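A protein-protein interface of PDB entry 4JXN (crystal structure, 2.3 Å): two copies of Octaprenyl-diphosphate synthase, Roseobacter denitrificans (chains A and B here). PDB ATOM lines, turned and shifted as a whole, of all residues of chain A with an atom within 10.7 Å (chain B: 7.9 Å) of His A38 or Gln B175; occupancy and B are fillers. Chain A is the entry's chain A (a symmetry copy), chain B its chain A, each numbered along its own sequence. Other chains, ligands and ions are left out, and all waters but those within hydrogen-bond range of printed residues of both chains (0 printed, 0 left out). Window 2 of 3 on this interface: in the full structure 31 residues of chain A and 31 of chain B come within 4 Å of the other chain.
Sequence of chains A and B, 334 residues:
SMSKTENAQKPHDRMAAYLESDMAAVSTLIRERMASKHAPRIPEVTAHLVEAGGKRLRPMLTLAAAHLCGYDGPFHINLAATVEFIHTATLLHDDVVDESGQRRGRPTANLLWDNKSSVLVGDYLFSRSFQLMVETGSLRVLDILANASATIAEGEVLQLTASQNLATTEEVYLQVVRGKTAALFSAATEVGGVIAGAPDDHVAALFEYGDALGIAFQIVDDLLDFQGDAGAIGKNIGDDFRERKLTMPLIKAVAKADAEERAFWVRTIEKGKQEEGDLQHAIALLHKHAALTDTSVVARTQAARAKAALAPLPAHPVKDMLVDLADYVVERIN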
ATOM      1  N   GLU A  32     -31.841 -30.782  -0.498  1.00  0.00           N
ATOM      2  CA  GLU A  32     -32.495 -30.599  -1.817  1.00  0.00           C
ATOM      3  C   GLU A  32     -32.457 -29.145  -2.379  1.00  0.00           C
ATOM      4  O   GLU A  32     -32.439 -28.945  -3.597  1.00  0.00           O
ATOM      5  CB  GLU A  32     -33.943 -31.143  -1.759  1.00  0.00           C
ATOM      6  CG  GLU A  32     -34.984 -30.330  -2.518  1.00  0.00           C
ATOM      7  CD  GLU A  32     -36.395 -30.634  -2.057  1.00  0.00           C
ATOM      8  OE1 GLU A  32     -36.689 -31.824  -1.804  1.00  0.00           O
ATOM      9  OE2 GLU A  32     -37.201 -29.676  -1.943  1.00  0.00           O
ATOM     10  N   ARG A  33     -32.452 -28.139  -1.506  1.00  0.00           N
ATOM     11  CA  ARG A  33     -32.396 -26.736  -1.952  1.00  0.00           C
ATOM     12  C   ARG A  33     -30.975 -26.217  -2.143  1.00  0.00           C
ATOM     13  O   ARG A  33     -30.764 -25.251  -2.879  1.00  0.00           O
ATOM     14  CB  ARG A  33     -33.127 -25.817  -0.967  1.00  0.00           C
ATOM     15  CG  ARG A  33     -34.619 -26.064  -0.827  1.00  0.00           C
ATOM     16  CD  ARG A  33     -35.301 -26.212  -2.169  1.00  0.00           C
ATOM     17  NE  ARG A  33     -36.749 -26.366  -2.033  1.00  0.00           N
ATOM     18  CZ  ARG A  33     -37.609 -25.371  -1.826  1.00  0.00           C
ATOM     19  NH1 ARG A  33     -37.190 -24.112  -1.707  1.00  0.00           N
ATOM     20  NH2 ARG A  33     -38.907 -25.638  -1.732  1.00  0.00           N
ATOM     21  N   MET A  34     -30.007 -26.833  -1.470  1.00  0.00           N
ATOM     22  CA  MET A  34     -28.599 -26.528  -1.711  1.00  0.00           C
ATOM     23  C   MET A  34     -28.185 -26.998  -3.115  1.00  0.00           C
ATOM     24  O   MET A  34     -27.214 -26.496  -3.685  1.00  0.00           O
ATOM     25  CB  MET A  34     -27.721 -27.174  -0.645  1.00  0.00           C
ATOM     26  N   ALA A  35     -28.932 -27.958  -3.664  1.00  0.00           N
ATOM     27  CA  ALA A  35     -28.770 -28.378  -5.056  1.00  0.00           C
ATOM     28  C   ALA A  35     -29.228 -27.275  -6.003  1.00  0.00           C
ATOM     29  O   ALA A  35     -30.392 -26.861  -5.975  1.00  0.00           O
ATOM     30  CB  ALA A  35     -29.557 -29.653  -5.329  1.00  0.00           C
ATOM     31  N   SER A  36     -28.306 -26.818  -6.845  1.00  0.00           N
ATOM     32  CA  SER A  36     -28.562 -25.730  -7.782  1.00  0.00           C
ATOM     33  C   SER A  36     -28.803 -26.270  -9.197  1.00  0.00           C
ATOM     34  O   SER A  36     -27.948 -26.969  -9.756  1.00  0.00           O
ATOM     35  CB  SER A  36     -27.379 -24.759  -7.771  1.00  0.00           C
ATOM     36  OG  SER A  36     -27.529 -23.748  -8.749  1.00  0.00           O
ATOM     37  N   LYS A  37     -29.967 -25.934  -9.762  1.00  0.00           N
ATOM     38  CA  LYS A  37     -30.369 -26.369 -11.109  1.00  0.00           C
ATOM     39  C   LYS A  37     -29.217 -26.317 -12.110  1.00  0.00           C
ATOM     40  O   LYS A  37     -28.855 -27.333 -12.710  1.00  0.00           O
ATOM     41  CB  LYS A  37     -31.519 -25.500 -11.628  1.00  0.00           C
ATOM     42  N   HIS A  38     -28.637 -25.129 -12.266  1.00  0.00           N
ATOM     43  CA  HIS A  38     -27.619 -24.883 -13.287  1.00  0.00           C
ATOM     44  C   HIS A  38     -26.193 -25.152 -12.795  1.00  0.00           C
ATOM     45  O   HIS A  38     -25.534 -26.069 -13.287  1.00  0.00           O
ATOM     46  CB  HIS A  38     -27.756 -23.453 -13.821  1.00  0.00           C
ATOM     47  CG  HIS A  38     -29.054 -23.200 -14.526  1.00  0.00           C
ATOM     48  ND1 HIS A  38     -29.150 -23.121 -15.899  1.00  0.00           N
ATOM     49  CD2 HIS A  38     -30.311 -23.023 -14.051  1.00  0.00           C
ATOM     50  CE1 HIS A  38     -30.407 -22.899 -16.239  1.00  0.00           C
ATOM     51  NE2 HIS A  38     -31.132 -22.836 -15.138  1.00  0.00           N
ATOM     52  N   ALA A  39     -25.721 -24.364 -11.827  1.00  0.00           N
ATOM     53  CA  ALA A  39     -24.341 -24.485 -11.330  1.00  0.00           C
ATOM     54  C   ALA A  39     -24.134 -25.767 -10.499  1.00  0.00           C
ATOM     55  O   ALA A  39     -24.878 -26.011  -9.552  1.00  0.00           O
ATOM     56  CB  ALA A  39     -23.966 -23.250 -10.510  1.00  0.00           C
ATOM     57  N   PRO A  40     -23.131 -26.599 -10.861  1.00  0.00           N
ATOM     58  CA  PRO A  40     -22.805 -27.764 -10.039  1.00  0.00           C
ATOM     59  C   PRO A  40     -21.668 -27.527  -9.027  1.00  0.00           C
ATOM     60  O   PRO A  40     -21.274 -28.464  -8.330  1.00  0.00           O
ATOM     61  CB  PRO A  40     -22.383 -28.802 -11.081  1.00  0.00           C
ATOM     62  CG  PRO A  40     -21.776 -27.999 -12.183  1.00  0.00           C
ATOM     63  CD  PRO A  40     -22.368 -26.610 -12.125  1.00  0.00           C
ATOM     64  N   ARG A  41     -21.166 -26.293  -8.934  1.00  0.00           N
ATOM     65  CA  ARG A  41     -20.015 -25.966  -8.072  1.00  0.00           C
ATOM     66  C   ARG A  41     -20.385 -25.568  -6.628  1.00  0.00           C
ATOM     67  O   ARG A  41     -19.525 -25.072  -5.878  1.00  0.00           O
ATOM     68  CB  ARG A  41     -19.190 -24.845  -8.715  1.00  0.00           C
ATOM     69  N   ILE A  42     -21.651 -25.778  -6.250  1.00  0.00           N
ATOM     70  CA  ILE A  42     -22.144 -25.472  -4.895  1.00  0.00           C
ATOM     71  C   ILE A  42     -22.139 -26.679  -3.942  1.00  0.00           C
ATOM     72  O   ILE A  42     -21.495 -26.608  -2.895  1.00  0.00           O
ATOM     73  CB  ILE A  42     -23.562 -24.833  -4.911  1.00  0.00           C
ATOM     74  CG1 ILE A  42     -23.553 -23.495  -5.663  1.00  0.00           C
ATOM     75  CG2 ILE A  42     -24.081 -24.630  -3.489  1.00  0.00           C
ATOM     76  CD1 ILE A  42     -23.714 -23.617  -7.165  1.00  0.00           C
ATOM     77  N   PRO A  43     -22.854 -27.780  -4.290  1.00  0.00           N
ATOM     78  CA  PRO A  43     -23.088 -28.878  -3.325  1.00  0.00           C
ATOM     79  C   PRO A  43     -21.853 -29.466  -2.608  1.00  0.00           C
ATOM     80  O   PRO A  43     -21.998 -30.050  -1.528  1.00  0.00           O
ATOM     81  CB  PRO A  43     -23.766 -29.958  -4.182  1.00  0.00           C
ATOM     82  CG  PRO A  43     -24.409 -29.209  -5.292  1.00  0.00           C
ATOM     83  CD  PRO A  43     -23.450 -28.098  -5.602  1.00  0.00           C
ATOM     84  N   TYR A 124     -26.257 -17.305  -1.794  1.00  0.00           N
ATOM     85  CA  TYR A 124     -27.097 -18.345  -2.367  1.00  0.00           C
ATOM     86  C   TYR A 124     -28.045 -18.932  -1.325  1.00  0.00           C
ATOM     87  O   TYR A 124     -29.233 -19.144  -1.603  1.00  0.00           O
ATOM     88  CB  TYR A 124     -26.253 -19.462  -3.014  1.00  0.00           C
ATOM     89  CG  TYR A 124     -27.105 -20.569  -3.622  1.00  0.00           C
ATOM     90  CD1 TYR A 124     -28.153 -20.265  -4.495  1.00  0.00           C
ATOM     91  CD2 TYR A 124     -26.887 -21.915  -3.306  1.00  0.00           C
ATOM     92  CE1 TYR A 124     -28.949 -21.257  -5.042  1.00  0.00           C
ATOM     93  CE2 TYR A 124     -27.681 -22.916  -3.853  1.00  0.00           C
ATOM     94  CZ  TYR A 124     -28.710 -22.577  -4.718  1.00  0.00           C
ATOM     95  OH  TYR A 124     -29.510 -23.544  -5.270  1.00  0.00           O
ATOM     96  N   ARG A 128     -32.086 -18.808  -1.068  1.00  0.00           N
ATOM     97  CA  ARG A 128     -32.855 -20.034  -0.847  1.00  0.00           C
ATOM     98  C   ARG A 128     -33.716 -19.963   0.420  1.00  0.00           C
ATOM     99  O   ARG A 128     -34.857 -20.433   0.424  1.00  0.00           O
ATOM    100  CB  ARG A 128     -31.927 -21.243  -0.788  1.00  0.00           C
ATOM    101  CG  ARG A 128     -31.323 -21.604  -2.134  1.00  0.00           C
ATOM    102  CD  ARG A 128     -32.302 -22.388  -2.986  1.00  0.00           C
ATOM    103  NE  ARG A 128     -31.977 -22.289  -4.405  1.00  0.00           N
ATOM    104  CZ  ARG A 128     -32.501 -23.060  -5.354  1.00  0.00           C
ATOM    105  NH1 ARG A 128     -33.393 -24.003  -5.055  1.00  0.00           N
ATOM    106  NH2 ARG A 128     -32.127 -22.886  -6.618  1.00  0.00           N
ATOM    107  N   THR B 151     -31.733 -16.699  -8.870  1.00  0.00           N
ATOM    108  CA  THR B 151     -31.069 -16.674 -10.175  1.00  0.00           C
ATOM    109  C   THR B 151     -29.774 -15.855 -10.121  1.00  0.00           C
ATOM    110  O   THR B 151     -28.719 -16.304 -10.587  1.00  0.00           O
ATOM    111  CB  THR B 151     -32.014 -16.161 -11.278  1.00  0.00           C
ATOM    112  OG1 THR B 151     -33.230 -16.921 -11.247  1.00  0.00           O
ATOM    113  CG2 THR B 151     -31.380 -16.312 -12.661  1.00  0.00           C
ATOM    114  N   ILE B 152     -29.837 -14.678  -9.513  1.00  0.00           N
ATOM    115  CA  ILE B 152     -28.669 -13.800  -9.477  1.00  0.00           C
ATOM    116  C   ILE B 152     -27.497 -14.495  -8.801  1.00  0.00           C
ATOM    117  O   ILE B 152     -26.411 -14.630  -9.389  1.00  0.00           O
ATOM    118  CB  ILE B 152     -28.972 -12.473  -8.761  1.00  0.00           C
ATOM    119  CG1 ILE B 152     -29.963 -11.649  -9.590  1.00  0.00           C
ATOM    120  CG2 ILE B 152     -27.691 -11.672  -8.526  1.00  0.00           C
ATOM    121  CD1 ILE B 152     -30.816 -10.717  -8.762  1.00  0.00           C
ATOM    122  N   GLU B 154     -27.075 -17.575  -8.181  1.00  0.00           N
ATOM    123  CA  GLU B 154     -26.759 -18.791  -8.934  1.00  0.00           C
ATOM    124  C   GLU B 154     -25.877 -18.514 -10.144  1.00  0.00           C
ATOM    125  O   GLU B 154     -25.035 -19.335 -10.496  1.00  0.00           O
ATOM    126  CB  GLU B 154     -28.062 -19.452  -9.392  1.00  0.00           C
ATOM    127  CG  GLU B 154     -27.899 -20.819 -10.024  1.00  0.00           C
ATOM    128  CD  GLU B 154     -29.224 -21.554 -10.217  1.00  0.00           C
ATOM    129  OE1 GLU B 154     -30.217 -21.246  -9.520  1.00  0.00           O
ATOM    130  OE2 GLU B 154     -29.271 -22.466 -11.069  1.00  0.00           O
ATOM    131  N   GLY B 155     -26.095 -17.374 -10.793  1.00  0.00           N
ATOM    132  CA  GLY B 155     -25.226 -16.933 -11.872  1.00  0.00           C
ATOM    133  C   GLY B 155     -23.835 -16.600 -11.369  1.00  0.00           C
ATOM    134  O   GLY B 155     -22.847 -17.072 -11.928  1.00  0.00           O
ATOM    135  N   GLU B 156     -23.766 -15.791 -10.308  1.00  0.00           N
ATOM    136  CA  GLU B 156     -22.492 -15.390  -9.689  1.00  0.00           C
ATOM    137  C   GLU B 156     -21.549 -16.586  -9.472  1.00  0.00           C
ATOM    138  O   GLU B 156     -20.345 -16.491  -9.714  1.00  0.00           O
ATOM    139  CB  GLU B 156     -22.733 -14.658  -8.352  1.00  0.00           C
ATOM    140  CG  GLU B 156     -23.294 -13.237  -8.461  1.00  0.00           C
ATOM    141  CD  GLU B 156     -23.518 -12.562  -7.101  1.00  0.00           C
ATOM    142  OE1 GLU B 156     -24.115 -13.178  -6.190  1.00  0.00           O
ATOM    143  OE2 GLU B 156     -23.108 -11.395  -6.933  1.00  0.00           O
ATOM    144  N   LEU B 158     -21.972 -19.718 -10.969  1.00  0.00           N
ATOM    145  CA  LEU B 158     -21.754 -20.263 -12.309  1.00  0.00           C
ATOM    146  C   LEU B 158     -20.653 -19.495 -13.031  1.00  0.00           C
ATOM    147  O   LEU B 158     -19.899 -20.062 -13.817  1.00  0.00           O
ATOM    148  CB  LEU B 158     -23.043 -20.210 -13.133  1.00  0.00           C
ATOM    149  CG  LEU B 158     -23.019 -20.806 -14.549  1.00  0.00           C
ATOM    150  CD1 LEU B 158     -22.586 -22.265 -14.539  1.00  0.00           C
ATOM    151  CD2 LEU B 158     -24.382 -20.667 -15.216  1.00  0.00           C
ATOM    152  N   GLN B 159     -20.562 -18.203 -12.751  1.00  0.00           N
ATOM    153  CA  GLN B 159     -19.520 -17.374 -13.319  1.00  0.00           C
ATOM    154  C   GLN B 159     -18.145 -17.863 -12.874  1.00  0.00           C
ATOM    155  O   GLN B 159     -17.231 -17.946 -13.692  1.00  0.00           O
ATOM    156  CB  GLN B 159     -19.725 -15.911 -12.922  1.00  0.00           C
ATOM    157  CG  GLN B 159     -19.041 -14.923 -13.851  1.00  0.00           C
ATOM    158  CD  GLN B 159     -19.265 -13.479 -13.449  1.00  0.00           C
ATOM    159  OE1 GLN B 159     -18.578 -12.575 -13.931  1.00  0.00           O
ATOM    160  NE2 GLN B 159     -20.228 -13.251 -12.561  1.00  0.00           N
ATOM    161  N   THR B 161     -17.010 -20.783 -12.190  1.00  0.00           N
ATOM    162  CA  THR B 161     -16.626 -21.966 -12.952  1.00  0.00           C
ATOM    163  C   THR B 161     -16.422 -21.641 -14.434  1.00  0.00           C
ATOM    164  O   THR B 161     -15.394 -21.983 -15.017  1.00  0.00           O
ATOM    165  CB  THR B 161     -17.695 -23.071 -12.822  1.00  0.00           C
ATOM    166  OG1 THR B 161     -18.912 -22.638 -13.438  1.00  0.00           O
ATOM    167  CG2 THR B 161     -17.972 -23.398 -11.353  1.00  0.00           C
ATOM    168  N   THR B 169     -20.093 -22.689 -23.883  1.00  0.00           N
ATOM    169  CA  THR B 169     -20.832 -22.278 -25.075  1.00  0.00           C
ATOM    170  C   THR B 169     -21.449 -20.899 -24.860  1.00  0.00           C
ATOM    171  O   THR B 169     -21.421 -20.357 -23.752  1.00  0.00           O
ATOM    172  CB  THR B 169     -21.962 -23.270 -25.427  1.00  0.00           C
ATOM    173  OG1 THR B 169     -22.742 -23.554 -24.257  1.00  0.00           O
ATOM    174  CG2 THR B 169     -21.386 -24.561 -25.988  1.00  0.00           C
ATOM    175  N   GLU B 170     -21.980 -20.324 -25.934  1.00  0.00           N
ATOM    176  CA  GLU B 170     -22.757 -19.096 -25.837  1.00  0.00           C
ATOM    177  C   GLU B 170     -24.018 -19.324 -25.031  1.00  0.00           C
ATOM    178  O   GLU B 170     -24.412 -18.468 -24.238  1.00  0.00           O
ATOM    179  CB  GLU B 170     -23.161 -18.598 -27.216  1.00  0.00           C
ATOM    180  CG  GLU B 170     -22.074 -17.855 -27.950  1.00  0.00           C
ATOM    181  CD  GLU B 170     -22.626 -17.169 -29.167  1.00  0.00           C
ATOM    182  OE1 GLU B 170     -23.236 -16.094 -28.995  1.00  0.00           O
ATOM    183  OE2 GLU B 170     -22.466 -17.723 -30.278  1.00  0.00           O
ATOM    184  N   GLU B 171     -24.655 -20.473 -25.246  1.00  0.00           N
ATOM    185  CA  GLU B 171     -25.879 -20.807 -24.526  1.00  0.00           C
ATOM    186  C   GLU B 171     -25.643 -20.804 -23.013  1.00  0.00           C
ATOM    187  O   GLU B 171     -26.533 -20.454 -22.250  1.00  0.00           O
ATOM    188  CB  GLU B 171     -26.418 -22.163 -24.979  1.00  0.00           C
ATOM    189  CG  GLU B 171     -27.839 -22.446 -24.507  1.00  0.00           C
ATOM    190  CD  GLU B 171     -28.217 -23.907 -24.646  1.00  0.00           C
ATOM    191  OE1 GLU B 171     -28.222 -24.624 -23.618  1.00  0.00           O
ATOM    192  OE2 GLU B 171     -28.492 -24.342 -25.783  1.00  0.00           O
ATOM    193  N   VAL B 172     -24.439 -21.184 -22.594  1.00  0.00           N
ATOM    194  CA  VAL B 172     -24.053 -21.150 -21.186  1.00  0.00           C
ATOM    195  C   VAL B 172     -23.743 -19.739 -20.709  1.00  0.00           C
ATOM    196  O   VAL B 172     -23.939 -19.414 -19.533  1.00  0.00           O
ATOM    197  CB  VAL B 172     -22.813 -22.037 -20.931  1.00  0.00           C
ATOM    198  CG1 VAL B 172     -22.264 -21.826 -19.521  1.00  0.00           C
ATOM    199  CG2 VAL B 172     -23.152 -23.503 -21.162  1.00  0.00           C
ATOM    200  N   TYR B 173     -23.219 -18.907 -21.602  1.00  0.00           N
ATOM    201  CA  TYR B 173     -22.952 -17.511 -21.258  1.00  0.00           C
ATOM    202  C   TYR B 173     -24.268 -16.745 -21.040  1.00  0.00           C
ATOM    203  O   TYR B 173     -24.362 -15.903 -20.136  1.00  0.00           O
ATOM    204  CB  TYR B 173     -22.090 -16.828 -22.335  1.00  0.00           C
ATOM    205  CG  TYR B 173     -21.747 -15.392 -21.995  1.00  0.00           C
ATOM    206  CD1 TYR B 173     -21.068 -15.084 -20.815  1.00  0.00           C
ATOM    207  CD2 TYR B 173     -22.133 -14.338 -22.829  1.00  0.00           C
ATOM    208  CE1 TYR B 173     -20.771 -13.773 -20.476  1.00  0.00           C
ATOM    209  CE2 TYR B 173     -21.838 -13.018 -22.496  1.00  0.00           C
ATOM    210  CZ  TYR B 173     -21.157 -12.740 -21.319  1.00  0.00           C
ATOM    211  OH  TYR B 173     -20.859 -11.432 -20.966  1.00  0.00           O
ATOM    212  N   LEU B 174     -25.277 -17.042 -21.862  1.00  0.00           N
ATOM    213  CA  LEU B 174     -26.607 -16.410 -21.737  1.00  0.00           C
ATOM    214  C   LEU B 174     -27.222 -16.639 -20.353  1.00  0.00           C
ATOM    215  O   LEU B 174     -27.831 -15.729 -19.789  1.00  0.00           O
ATOM    216  CB  LEU B 174     -27.550 -16.898 -22.846  1.00  0.00           C
ATOM    217  CG  LEU B 174     -27.532 -16.156 -24.200  1.00  0.00           C
ATOM    218  CD1 LEU B 174     -26.206 -15.465 -24.525  1.00  0.00           C
ATOM    219  CD2 LEU B 174     -27.939 -17.096 -25.334  1.00  0.00           C
ATOM    220  N   GLN B 175     -27.018 -17.839 -19.806  1.00  0.00           N
ATOM    221  CA  GLN B 175     -27.403 -18.161 -18.423  1.00  0.00           C
ATOM    222  C   GLN B 175     -26.660 -17.288 -17.436  1.00  0.00           C
ATOM    223  O   GLN B 175     -27.247 -16.763 -16.497  1.00  0.00           O
ATOM    224  CB  GLN B 175     -27.117 -19.629 -18.099  1.00  0.00           C
ATOM    225  CG  GLN B 175     -27.957 -20.618 -18.893  1.00  0.00           C
ATOM    226  CD  GLN B 175     -27.491 -22.056 -18.744  1.00  0.00           C
ATOM    227  OE1 GLN B 175     -26.380 -22.330 -18.280  1.00  0.00           O
ATOM    228  NE2 GLN B 175     -28.346 -22.989 -19.143  1.00  0.00           N
ATOM    229  N   VAL B 176     -25.368 -17.110 -17.665  1.00  0.00           N
ATOM    230  CA  VAL B 176     -24.565 -16.246 -16.797  1.00  0.00           C
ATOM    231  C   VAL B 176     -25.091 -14.812 -16.844  1.00  0.00           C
ATOM    232  O   VAL B 176     -25.179 -14.130 -15.826  1.00  0.00           O
ATOM    233  CB  VAL B 176     -23.069 -16.261 -17.203  1.00  0.00           C
ATOM    234  CG1 VAL B 176     -22.262 -15.272 -16.368  1.00  0.00           C
ATOM    235  CG2 VAL B 176     -22.483 -17.666 -17.082  1.00  0.00           C
ATOM    236  N   VAL B 177     -25.431 -14.371 -18.049  1.00  0.00           N
ATOM    237  CA  VAL B 177     -25.920 -13.019 -18.289  1.00  0.00           C
ATOM    238  C   VAL B 177     -27.253 -12.773 -17.585  1.00  0.00           C
ATOM    239  O   VAL B 177     -27.440 -11.727 -16.945  1.00  0.00           O
ATOM    240  CB  VAL B 177     -26.064 -12.773 -19.808  1.00  0.00           C
ATOM    241  CG1 VAL B 177     -26.906 -11.543 -20.093  1.00  0.00           C
ATOM    242  CG2 VAL B 177     -24.680 -12.643 -20.441  1.00  0.00           C
ATOM    243  N   ARG B 178     -28.172 -13.732 -17.711  1.00  0.00           N
ATOM    244  CA  ARG B 178     -29.449 -13.654 -17.012  1.00  0.00           C
ATOM    245  C   ARG B 178     -29.235 -13.475 -15.515  1.00  0.00           C
ATOM    246  O   ARG B 178     -29.733 -12.522 -14.913  1.00  0.00           O
ATOM    247  CB  ARG B 178     -30.282 -14.897 -17.279  1.00  0.00           C
ATOM    248  CG  ARG B 178     -30.710 -15.037 -18.736  1.00  0.00           C
ATOM    249  CD  ARG B 178     -32.117 -15.573 -18.840  1.00  0.00           C
ATOM    250  NE  ARG B 178     -32.733 -15.285 -20.126  1.00  0.00           N
ATOM    251  CZ  ARG B 178     -32.464 -15.928 -21.259  1.00  0.00           C
ATOM    252  NH1 ARG B 178     -33.108 -15.580 -22.366  1.00  0.00           N
ATOM    253  NH2 ARG B 178     -31.559 -16.905 -21.305  1.00  0.00           N
ATOM    254  N   GLY B 179     -28.461 -14.375 -14.925  1.00  0.00           N
ATOM    255  CA  GLY B 179     -28.170 -14.295 -13.504  1.00  0.00           C
ATOM    256  C   GLY B 179     -27.559 -12.963 -13.124  1.00  0.00           C
ATOM    257  O   GLY B 179     -28.160 -12.170 -12.398  1.00  0.00           O
ATOM    258  N   LYS B 180     -26.368 -12.703 -13.642  1.00  0.00           N
ATOM    259  CA  LYS B 180     -25.622 -11.520 -13.250  1.00  0.00           C
ATOM    260  C   LYS B 180     -26.349 -10.222 -13.614  1.00  0.00           C
ATOM    261  O   LYS B 180     -26.233  -9.235 -12.882  1.00  0.00           O
ATOM    262  CB  LYS B 180     -24.209 -11.542 -13.860  1.00  0.00           C
ATOM    263  CG  LYS B 180     -24.130 -11.099 -15.314  1.00  0.00           C
ATOM    264  CD  LYS B 180     -22.822 -11.491 -15.990  1.00  0.00           C
ATOM    265  CE  LYS B 180     -21.593 -10.891 -15.314  1.00  0.00           C
ATOM    266  NZ  LYS B 180     -21.700  -9.426 -15.055  1.00  0.00           N
ATOM    267  N   THR B 181     -27.099 -10.218 -14.722  1.00  0.00           N
ATOM    268  CA  THR B 181     -27.695  -8.970 -15.223  1.00  0.00           C
ATOM    269  C   THR B 181     -29.209  -8.991 -15.446  1.00  0.00           C
ATOM    270  O   THR B 181     -29.923  -8.172 -14.868  1.00  0.00           O
ATOM    271  CB  THR B 181     -27.025  -8.516 -16.538  1.00  0.00           C
ATOM    272  OG1 THR B 181     -25.605  -8.488 -16.372  1.00  0.00           O
ATOM    273  CG2 THR B 181     -27.491  -7.117 -16.938  1.00  0.00           C
ATOM    274  N   ALA B 182     -29.699  -9.888 -16.300  1.00  0.00           N
ATOM    275  CA  ALA B 182     -31.058  -9.719 -16.833  1.00  0.00           C
ATOM    276  C   ALA B 182     -32.153 -10.008 -15.803  1.00  0.00           C
ATOM    277  O   ALA B 182     -33.206  -9.375 -15.824  1.00  0.00           O
ATOM    278  CB  ALA B 182     -31.262 -10.559 -18.088  1.00  0.00           C
ATOM    279  N   ALA B 183     -31.896 -10.952 -14.906  1.00  0.00           N
ATOM    280  CA  ALA B 183     -32.888 -11.377 -13.920  1.00  0.00           C
ATOM    281  C   ALA B 183     -33.448 -10.206 -13.125  1.00  0.00           C
ATOM    282  O   ALA B 183     -34.672 -10.135 -12.902  1.00  0.00           O
ATOM    283  CB  ALA B 183     -32.309 -12.425 -12.983  1.00  0.00           C
ATOM    284  N   ILE B 215     -30.186  -8.515 -21.271  1.00  0.00           N
ATOM    285  CA  ILE B 215     -29.253  -9.258 -22.107  1.00  0.00           C
ATOM    286  C   ILE B 215     -28.552  -8.301 -23.067  1.00  0.00           C
ATOM    287  O   ILE B 215     -27.325  -8.336 -23.189  1.00  0.00           O
ATOM    288  CB  ILE B 215     -29.944 -10.422 -22.868  1.00  0.00           C
ATOM    289  CG1 ILE B 215     -30.493 -11.462 -21.882  1.00  0.00           C
ATOM    290  CG2 ILE B 215     -28.947 -11.128 -23.780  1.00  0.00           C
ATOM    291  CD1 ILE B 215     -31.486 -12.439 -22.488  1.00  0.00           C
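Glu B154 touches Lys A37 (OE2 to N, 3.8 Å).
Arg A41 touches Thr B161.
Of the 14 printed residues of chain A, 5 touch a printed residue of chain B.
Printed residues of chain A that touch a printed residue of chain B: Ser A36, Lys A37, His A38, Arg A41 and Arg A128.
Along chain B the printed residues that touch a printed residue of chain A span positions 154 to 175.
Among the printed residues, 6 pairs touch across the chains.
Of chain B, only Glu B154 (3.0 Å) and Gln B175 (3.3 Å) come within 4 Å of His A38.
Of chain A, only His A38 (3.3 Å) comes within 4 Å of Gln B175.
Lys A37 touches just one residue of chain B: Glu B154.
Ala A39 touches none of the printed residues of chain B.
No residue of chain A comes within 4 Å of Gly B155.
No residue of chain A comes within 4 Å of Val B176.
No residue of chain A comes within 4 Å of Val B177.
No residue of chain A comes within 4 Å of Gly B179.
Of the printed residues of chain A, Thr B161 touches Arg A41.
Of the printed residues of chain B, Ser A36 touches Glu B154.
Printed residues of chain B within 4 Å of Arg A41: Thr B161.
Of the printed residues of chain A, Glu B154 touches Ser A36, Lys A37, His A38 and Arg A128.
The nearest residue of chain A that does not touch Gln B175 is Ala A39 (6.8 Å).
A ring nitrogen (ND1) of His A38 sits at hydrogen-bond distance from the side-chain amide nitrogen of Gln B175, at 3.3 Å.
The backbone NH of His A38 sits at hydrogen-bond distance from the side-chain carboxylate of Glu B154.
The side-chain carboxylate (OE1) of Glu B154 lies within salt-bridge range of the guanidinium group (NH2) of Arg A128, at 3.8 Å.
OE2 of Glu B154 sits close to OG of Ser A36, at 3.2 Å.
No position is printed for both chains.
Of the 6 pairs that touch across the chains among the printed residues, none has its exchanged pair printed and touching as well.
The guanidinium group (NE) of Arg A128 is in hydrogen-bond range of the side-chain hydroxyl (OH) of Tyr A124.
O of Leu B158 sits at hydrogen-bond distance from OG1 of Thr B161 (2.8 Å).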
